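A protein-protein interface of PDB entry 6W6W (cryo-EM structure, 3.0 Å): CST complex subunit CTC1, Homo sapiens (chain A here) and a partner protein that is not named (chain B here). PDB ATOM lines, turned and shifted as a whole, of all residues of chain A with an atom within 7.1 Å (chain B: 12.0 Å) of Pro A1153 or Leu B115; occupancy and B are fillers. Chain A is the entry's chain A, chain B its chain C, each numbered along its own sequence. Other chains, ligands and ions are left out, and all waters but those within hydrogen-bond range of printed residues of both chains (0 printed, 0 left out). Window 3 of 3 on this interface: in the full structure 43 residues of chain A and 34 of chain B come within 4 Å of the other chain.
Ser A1122 touches Gln B118. Leu B115 touches Pro A1153. Met A1154 touches Leu B115. Met A1156 touches Leu B119. CE1 of Phe A1157 touches O of Gln B118 (3.8 Å). CD1 of Phe A1157 touches CA of Leu B119, at 3.8 Å. Leu B122 touches Phe A1157 (CD2 to CE1, 3.8 Å).
Pro A1153 touches just one residue of chain B: Leu B115 (3.6 Å). Leu B115 touches two residues of chain A. Leu A1123 touches none of the printed residues of chain B. No residue of chain B comes within 4 Å of Phe A1126. Met A1154 touches just one residue of chain B: Leu B115. No residue of chain B comes within 4 Å of Thr A1155. Phe A1157 touches just these residues of chain B: Gln B118, Leu B119 and Leu B122. Printed residues of chain B within 4 Å of Met A1156: Leu B119 (3.8 Å). Of the printed residues of chain A, Leu B119 touches Met A1156 (3.8 Å) and Phe A1157 (3.8 Å). Of the printed residues of chain A, Gln B118 touches Ser A1122 and Phe A1157.
Of the 10 printed residues of chain B, 4 touch a printed residue of chain A. Hydrophobic or aromatic side chains of chain B that line the printed part of chain A: Leu B115, Leu B119 and Leu B122. Of the 11 printed residues of chain A, 5 touch a printed residue of chain B. Printed residues of chain A that touch a printed residue of chain B: Ser A1122, Pro A1153, Met A1154, Met A1156 and Phe A1157. Hydrophobic or aromatic side chains of chain A within 4 Å of the printed part of chain B: Pro A1153, Met A1154 and Phe A1157. Among the printed residues, 7 pairs touch across the chains. Among the printed residues, no Asp or Glu carboxylate lies within 4 Å of a Lys or Arg side-chain nitrogen of the other chain.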
ATOM      1  N   SER A1122      -1.194  26.631 -26.085  1.00  0.00           N
ATOM      2  CA  SER A1122       0.009  25.871 -26.391  1.00  0.00           C
ATOM      3  C   SER A1122      -0.047  24.460 -25.831  1.00  0.00           C
ATOM      4  O   SER A1122       0.686  23.591 -26.305  1.00  0.00           O
ATOM      5  CB  SER A1122       1.241  26.587 -25.850  1.00  0.00           C
ATOM      6  OG  SER A1122       1.232  26.605 -24.436  1.00  0.00           O
ATOM      7  N   LEU A1123      -0.873  24.221 -24.817  1.00  0.00           N
ATOM      8  CA  LEU A1123      -1.113  22.863 -24.351  1.00  0.00           C
ATOM      9  C   LEU A1123      -2.037  22.110 -25.293  1.00  0.00           C
ATOM     10  O   LEU A1123      -1.952  20.882 -25.399  1.00  0.00           O
ATOM     11  CB  LEU A1123      -1.706  22.901 -22.943  1.00  0.00           C
ATOM     12  CG  LEU A1123      -2.067  21.598 -22.229  1.00  0.00           C
ATOM     13  CD1 LEU A1123      -0.819  20.809 -21.887  1.00  0.00           C
ATOM     14  CD2 LEU A1123      -2.895  21.872 -20.989  1.00  0.00           C
ATOM     15  N   PHE A1126      -0.340  20.611 -28.623  1.00  0.00           N
ATOM     16  CA  PHE A1126       0.475  19.426 -28.399  1.00  0.00           C
ATOM     17  C   PHE A1126      -0.364  18.160 -28.450  1.00  0.00           C
ATOM     18  O   PHE A1126       0.171  17.080 -28.715  1.00  0.00           O
ATOM     19  CB  PHE A1126       1.184  19.520 -27.051  1.00  0.00           C
ATOM     20  CG  PHE A1126       2.589  20.038 -27.131  1.00  0.00           C
ATOM     21  CD1 PHE A1126       3.652  19.170 -27.313  1.00  0.00           C
ATOM     22  CD2 PHE A1126       2.849  21.390 -27.005  1.00  0.00           C
ATOM     23  CE1 PHE A1126       4.949  19.645 -27.378  1.00  0.00           C
ATOM     24  CE2 PHE A1126       4.139  21.873 -27.069  1.00  0.00           C
ATOM     25  CZ  PHE A1126       5.190  21.000 -27.255  1.00  0.00           C
ATOM     26  N   ASP A1151       4.097  10.520 -24.525  1.00  0.00           N
ATOM     27  CA  ASP A1151       3.755   9.887 -23.258  1.00  0.00           C
ATOM     28  C   ASP A1151       4.753  10.270 -22.175  1.00  0.00           C
ATOM     29  O   ASP A1151       4.463  10.154 -20.987  1.00  0.00           O
ATOM     30  CB  ASP A1151       3.701   8.364 -23.409  1.00  0.00           C
ATOM     31  CG  ASP A1151       2.824   7.703 -22.361  1.00  0.00           C
ATOM     32  OD1 ASP A1151       1.591   7.901 -22.407  1.00  0.00           O
ATOM     33  OD2 ASP A1151       3.362   6.986 -21.493  1.00  0.00           O
ATOM     34  N   GLU A1152       5.949  10.668 -22.582  1.00  0.00           N
ATOM     35  CA  GLU A1152       6.879  11.241 -21.615  1.00  0.00           C
ATOM     36  C   GLU A1152       6.610  12.726 -21.332  1.00  0.00           C
ATOM     37  O   GLU A1152       6.453  13.069 -20.154  1.00  0.00           O
ATOM     38  CB  GLU A1152       8.335  10.999 -22.043  1.00  0.00           C
ATOM     39  CG  GLU A1152       8.768   9.537 -22.009  1.00  0.00           C
ATOM     40  CD  GLU A1152       8.560   8.883 -20.656  1.00  0.00           C
ATOM     41  OE1 GLU A1152       8.885   9.512 -19.627  1.00  0.00           O
ATOM     42  OE2 GLU A1152       8.072   7.734 -20.621  1.00  0.00           O
ATOM     43  N   PRO A1153       6.548  13.671 -22.342  1.00  0.00           N
ATOM     44  CA  PRO A1153       6.350  15.079 -21.962  1.00  0.00           C
ATOM     45  C   PRO A1153       4.935  15.369 -21.489  1.00  0.00           C
ATOM     46  O   PRO A1153       4.742  16.014 -20.456  1.00  0.00           O
ATOM     47  CB  PRO A1153       6.681  15.848 -23.250  1.00  0.00           C
ATOM     48  CG  PRO A1153       7.343  14.864 -24.141  1.00  0.00           C
ATOM     49  CD  PRO A1153       6.676  13.584 -23.810  1.00  0.00           C
ATOM     50  N   MET A1154       3.938  14.900 -22.232  1.00  0.00           N
ATOM     51  CA  MET A1154       2.586  14.840 -21.709  1.00  0.00           C
ATOM     52  C   MET A1154       2.459  13.602 -20.831  1.00  0.00           C
ATOM     53  O   MET A1154       3.379  12.781 -20.765  1.00  0.00           O
ATOM     54  CB  MET A1154       1.567  14.828 -22.847  1.00  0.00           C
ATOM     55  CG  MET A1154       0.237  15.475 -22.504  1.00  0.00           C
ATOM     56  SD  MET A1154      -0.624  16.121 -23.943  1.00  0.00           S
ATOM     57  CE  MET A1154       0.046  17.775 -23.984  1.00  0.00           C
ATOM     58  N   THR A1155       1.366  13.554 -20.046  1.00  0.00           N
ATOM     59  CA  THR A1155       0.937  12.516 -19.094  1.00  0.00           C
ATOM     60  C   THR A1155       1.817  12.546 -17.833  1.00  0.00           C
ATOM     61  O   THR A1155       1.454  12.000 -16.785  1.00  0.00           O
ATOM     62  CB  THR A1155       0.910  11.128 -19.781  1.00  0.00           C
ATOM     63  OG1 THR A1155       0.147  11.225 -20.988  1.00  0.00           O
ATOM     64  CG2 THR A1155       0.230  10.056 -18.939  1.00  0.00           C
ATOM     65  N   MET A1156       2.921  13.287 -17.882  1.00  0.00           N
ATOM     66  CA  MET A1156       3.746  13.609 -16.733  1.00  0.00           C
ATOM     67  C   MET A1156       3.675  15.077 -16.376  1.00  0.00           C
ATOM     68  O   MET A1156       3.985  15.442 -15.244  1.00  0.00           O
ATOM     69  CB  MET A1156       5.208  13.233 -17.000  1.00  0.00           C
ATOM     70  CG  MET A1156       6.002  12.811 -15.771  1.00  0.00           C
ATOM     71  SD  MET A1156       5.637  11.139 -15.196  1.00  0.00           S
ATOM     72  CE  MET A1156       4.617  11.465 -13.760  1.00  0.00           C
ATOM     73  N   PHE A1157       3.289  15.925 -17.328  1.00  0.00           N
ATOM     74  CA  PHE A1157       2.965  17.306 -17.012  1.00  0.00           C
ATOM     75  C   PHE A1157       1.553  17.419 -16.463  1.00  0.00           C
ATOM     76  O   PHE A1157       1.301  18.211 -15.552  1.00  0.00           O
ATOM     77  CB  PHE A1157       3.118  18.183 -18.252  1.00  0.00           C
ATOM     78  CG  PHE A1157       2.554  19.560 -18.088  1.00  0.00           C
ATOM     79  CD1 PHE A1157       3.128  20.455 -17.207  1.00  0.00           C
ATOM     80  CD2 PHE A1157       1.443  19.957 -18.807  1.00  0.00           C
ATOM     81  CE1 PHE A1157       2.609  21.722 -17.051  1.00  0.00           C
ATOM     82  CE2 PHE A1157       0.920  21.223 -18.652  1.00  0.00           C
ATOM     83  CZ  PHE A1157       1.505  22.104 -17.774  1.00  0.00           C
ATOM     84  N   LEU A1158       0.624  16.628 -16.998  1.00  0.00           N
ATOM     85  CA  LEU A1158      -0.759  16.699 -16.552  1.00  0.00           C
ATOM     86  C   LEU A1158      -0.952  16.009 -15.212  1.00  0.00           C
ATOM     87  O   LEU A1158      -1.746  16.469 -14.388  1.00  0.00           O
ATOM     88  CB  LEU A1158      -1.680  16.087 -17.602  1.00  0.00           C
ATOM     89  CG  LEU A1158      -1.787  16.859 -18.914  1.00  0.00           C
ATOM     90  CD1 LEU A1158      -2.755  16.170 -19.849  1.00  0.00           C
ATOM     91  CD2 LEU A1158      -2.218  18.289 -18.658  1.00  0.00           C
ATOM     92  N   LEU B 115       7.078  21.966 -23.745  1.00  0.00           N
ATOM     93  CA  LEU B 115       6.257  21.290 -22.748  1.00  0.00           C
ATOM     94  C   LEU B 115       7.092  20.897 -21.543  1.00  0.00           C
ATOM     95  O   LEU B 115       6.576  20.788 -20.435  1.00  0.00           O
ATOM     96  CB  LEU B 115       5.582  20.055 -23.339  1.00  0.00           C
ATOM     97  CG  LEU B 115       4.327  19.575 -22.614  1.00  0.00           C
ATOM     98  CD1 LEU B 115       3.261  20.652 -22.610  1.00  0.00           C
ATOM     99  CD2 LEU B 115       3.797  18.308 -23.249  1.00  0.00           C
ATOM    100  N   THR B 116       8.387  20.678 -21.761  1.00  0.00           N
ATOM    101  CA  THR B 116       9.292  20.451 -20.642  1.00  0.00           C
ATOM    102  C   THR B 116       9.787  21.753 -20.030  1.00  0.00           C
ATOM    103  O   THR B 116      10.389  21.724 -18.954  1.00  0.00           O
ATOM    104  CB  THR B 116      10.482  19.590 -21.078  1.00  0.00           C
ATOM    105  OG1 THR B 116      11.170  19.111 -19.919  1.00  0.00           O
ATOM    106  CG2 THR B 116      11.450  20.389 -21.932  1.00  0.00           C
ATOM    107  N   SER B 117       9.551  22.884 -20.693  1.00  0.00           N
ATOM    108  CA  SER B 117       9.774  24.187 -20.089  1.00  0.00           C
ATOM    109  C   SER B 117       8.614  24.614 -19.207  1.00  0.00           C
ATOM    110  O   SER B 117       8.790  25.487 -18.352  1.00  0.00           O
ATOM    111  CB  SER B 117      10.004  25.239 -21.172  1.00  0.00           C
ATOM    112  OG  SER B 117      10.135  26.530 -20.605  1.00  0.00           O
ATOM    113  N   GLN B 118       7.437  24.028 -19.407  1.00  0.00           N
ATOM    114  CA  GLN B 118       6.284  24.296 -18.563  1.00  0.00           C
ATOM    115  C   GLN B 118       6.229  23.379 -17.353  1.00  0.00           C
ATOM    116  O   GLN B 118       5.757  23.797 -16.292  1.00  0.00           O
ATOM    117  CB  GLN B 118       4.994  24.145 -19.371  1.00  0.00           C
ATOM    118  CG  GLN B 118       4.437  25.442 -19.914  1.00  0.00           C
ATOM    119  CD  GLN B 118       3.058  25.267 -20.511  1.00  0.00           C
ATOM    120  OE1 GLN B 118       2.915  24.870 -21.666  1.00  0.00           O
ATOM    121  NE2 GLN B 118       2.030  25.555 -19.724  1.00  0.00           N
ATOM    122  N   LEU B 119       6.694  22.136 -17.493  1.00  0.00           N
ATOM    123  CA  LEU B 119       6.712  21.216 -16.363  1.00  0.00           C
ATOM    124  C   LEU B 119       7.801  21.579 -15.366  1.00  0.00           C
ATOM    125  O   LEU B 119       7.609  21.414 -14.157  1.00  0.00           O
ATOM    126  CB  LEU B 119       6.893  19.782 -16.865  1.00  0.00           C
ATOM    127  CG  LEU B 119       7.384  18.680 -15.922  1.00  0.00           C
ATOM    128  CD1 LEU B 119       6.345  18.365 -14.871  1.00  0.00           C
ATOM    129  CD2 LEU B 119       7.730  17.434 -16.705  1.00  0.00           C
ATOM    130  N   LYS B 120       8.936  22.088 -15.847  1.00  0.00           N
ATOM    131  CA  LYS B 120      10.043  22.415 -14.954  1.00  0.00           C
ATOM    132  C   LYS B 120       9.718  23.622 -14.088  1.00  0.00           C
ATOM    133  O   LYS B 120       9.922  23.592 -12.872  1.00  0.00           O
ATOM    134  CB  LYS B 120      11.316  22.653 -15.763  1.00  0.00           C
ATOM    135  CG  LYS B 120      12.180  21.415 -15.901  1.00  0.00           C
ATOM    136  CD  LYS B 120      13.386  21.670 -16.780  1.00  0.00           C
ATOM    137  CE  LYS B 120      14.026  20.365 -17.215  1.00  0.00           C
ATOM    138  NZ  LYS B 120      14.872  20.547 -18.425  1.00  0.00           N
ATOM    139  N   LYS B 121       9.183  24.685 -14.688  1.00  0.00           N
ATOM    140  CA  LYS B 121       8.812  25.862 -13.912  1.00  0.00           C
ATOM    141  C   LYS B 121       7.550  25.652 -13.084  1.00  0.00           C
ATOM    142  O   LYS B 121       7.254  26.482 -12.219  1.00  0.00           O
ATOM    143  CB  LYS B 121       8.638  27.067 -14.835  1.00  0.00           C
ATOM    144  CG  LYS B 121       7.266  27.198 -15.456  1.00  0.00           C
ATOM    145  CD  LYS B 121       7.146  28.506 -16.213  1.00  0.00           C
ATOM    146  CE  LYS B 121       7.304  29.693 -15.281  1.00  0.00           C
ATOM    147  NZ  LYS B 121       6.263  29.704 -14.218  1.00  0.00           N
ATOM    148  N   LEU B 122       6.804  24.575 -13.325  1.00  0.00           N
ATOM    149  CA  LEU B 122       5.716  24.209 -12.428  1.00  0.00           C
ATOM    150  C   LEU B 122       6.255  23.567 -11.157  1.00  0.00           C
ATOM    151  O   LEU B 122       5.695  23.761 -10.072  1.00  0.00           O
ATOM    152  CB  LEU B 122       4.750  23.271 -13.150  1.00  0.00           C
ATOM    153  CG  LEU B 122       3.768  22.408 -12.360  1.00  0.00           C
ATOM    154  CD1 LEU B 122       2.709  23.272 -11.719  1.00  0.00           C
ATOM    155  CD2 LEU B 122       3.137  21.366 -13.258  1.00  0.00           C
ATOM    156  N   GLN B 123       7.356  22.824 -11.265  1.00  0.00           N
ATOM    157  CA  GLN B 123       7.928  22.163 -10.098  1.00  0.00           C
ATOM    158  C   GLN B 123       8.650  23.130  -9.173  1.00  0.00           C
ATOM    159  O   GLN B 123       8.855  22.803  -8.001  1.00  0.00           O
ATOM    160  CB  GLN B 123       8.880  21.054 -10.535  1.00  0.00           C
ATOM    161  CG  GLN B 123       8.183  19.843 -11.111  1.00  0.00           C
ATOM    162  CD  GLN B 123       9.154  18.824 -11.665  1.00  0.00           C
ATOM    163  OE1 GLN B 123       8.942  17.619 -11.544  1.00  0.00           O
ATOM    164  NE2 GLN B 123      10.227  19.304 -12.279  1.00  0.00           N
ATOM    165  N   GLU B 124       9.047  24.301  -9.664  1.00  0.00           N
ATOM    166  CA  GLU B 124       9.566  25.353  -8.802  1.00  0.00           C
ATOM    167  C   GLU B 124       8.475  26.274  -8.293  1.00  0.00           C
ATOM    168  O   GLU B 124       8.780  27.283  -7.651  1.00  0.00           O
ATOM    169  CB  GLU B 124      10.638  26.178  -9.520  1.00  0.00           C
ATOM    170  CG  GLU B 124      11.993  25.499  -9.611  1.00  0.00           C
ATOM    171  CD  GLU B 124      12.097  24.529 -10.761  1.00  0.00           C
ATOM    172  OE1 GLU B 124      12.078  23.306 -10.516  1.00  0.00           O
ATOM    173  OE2 GLU B 124      12.237  24.996 -11.909  1.00  0.00           O
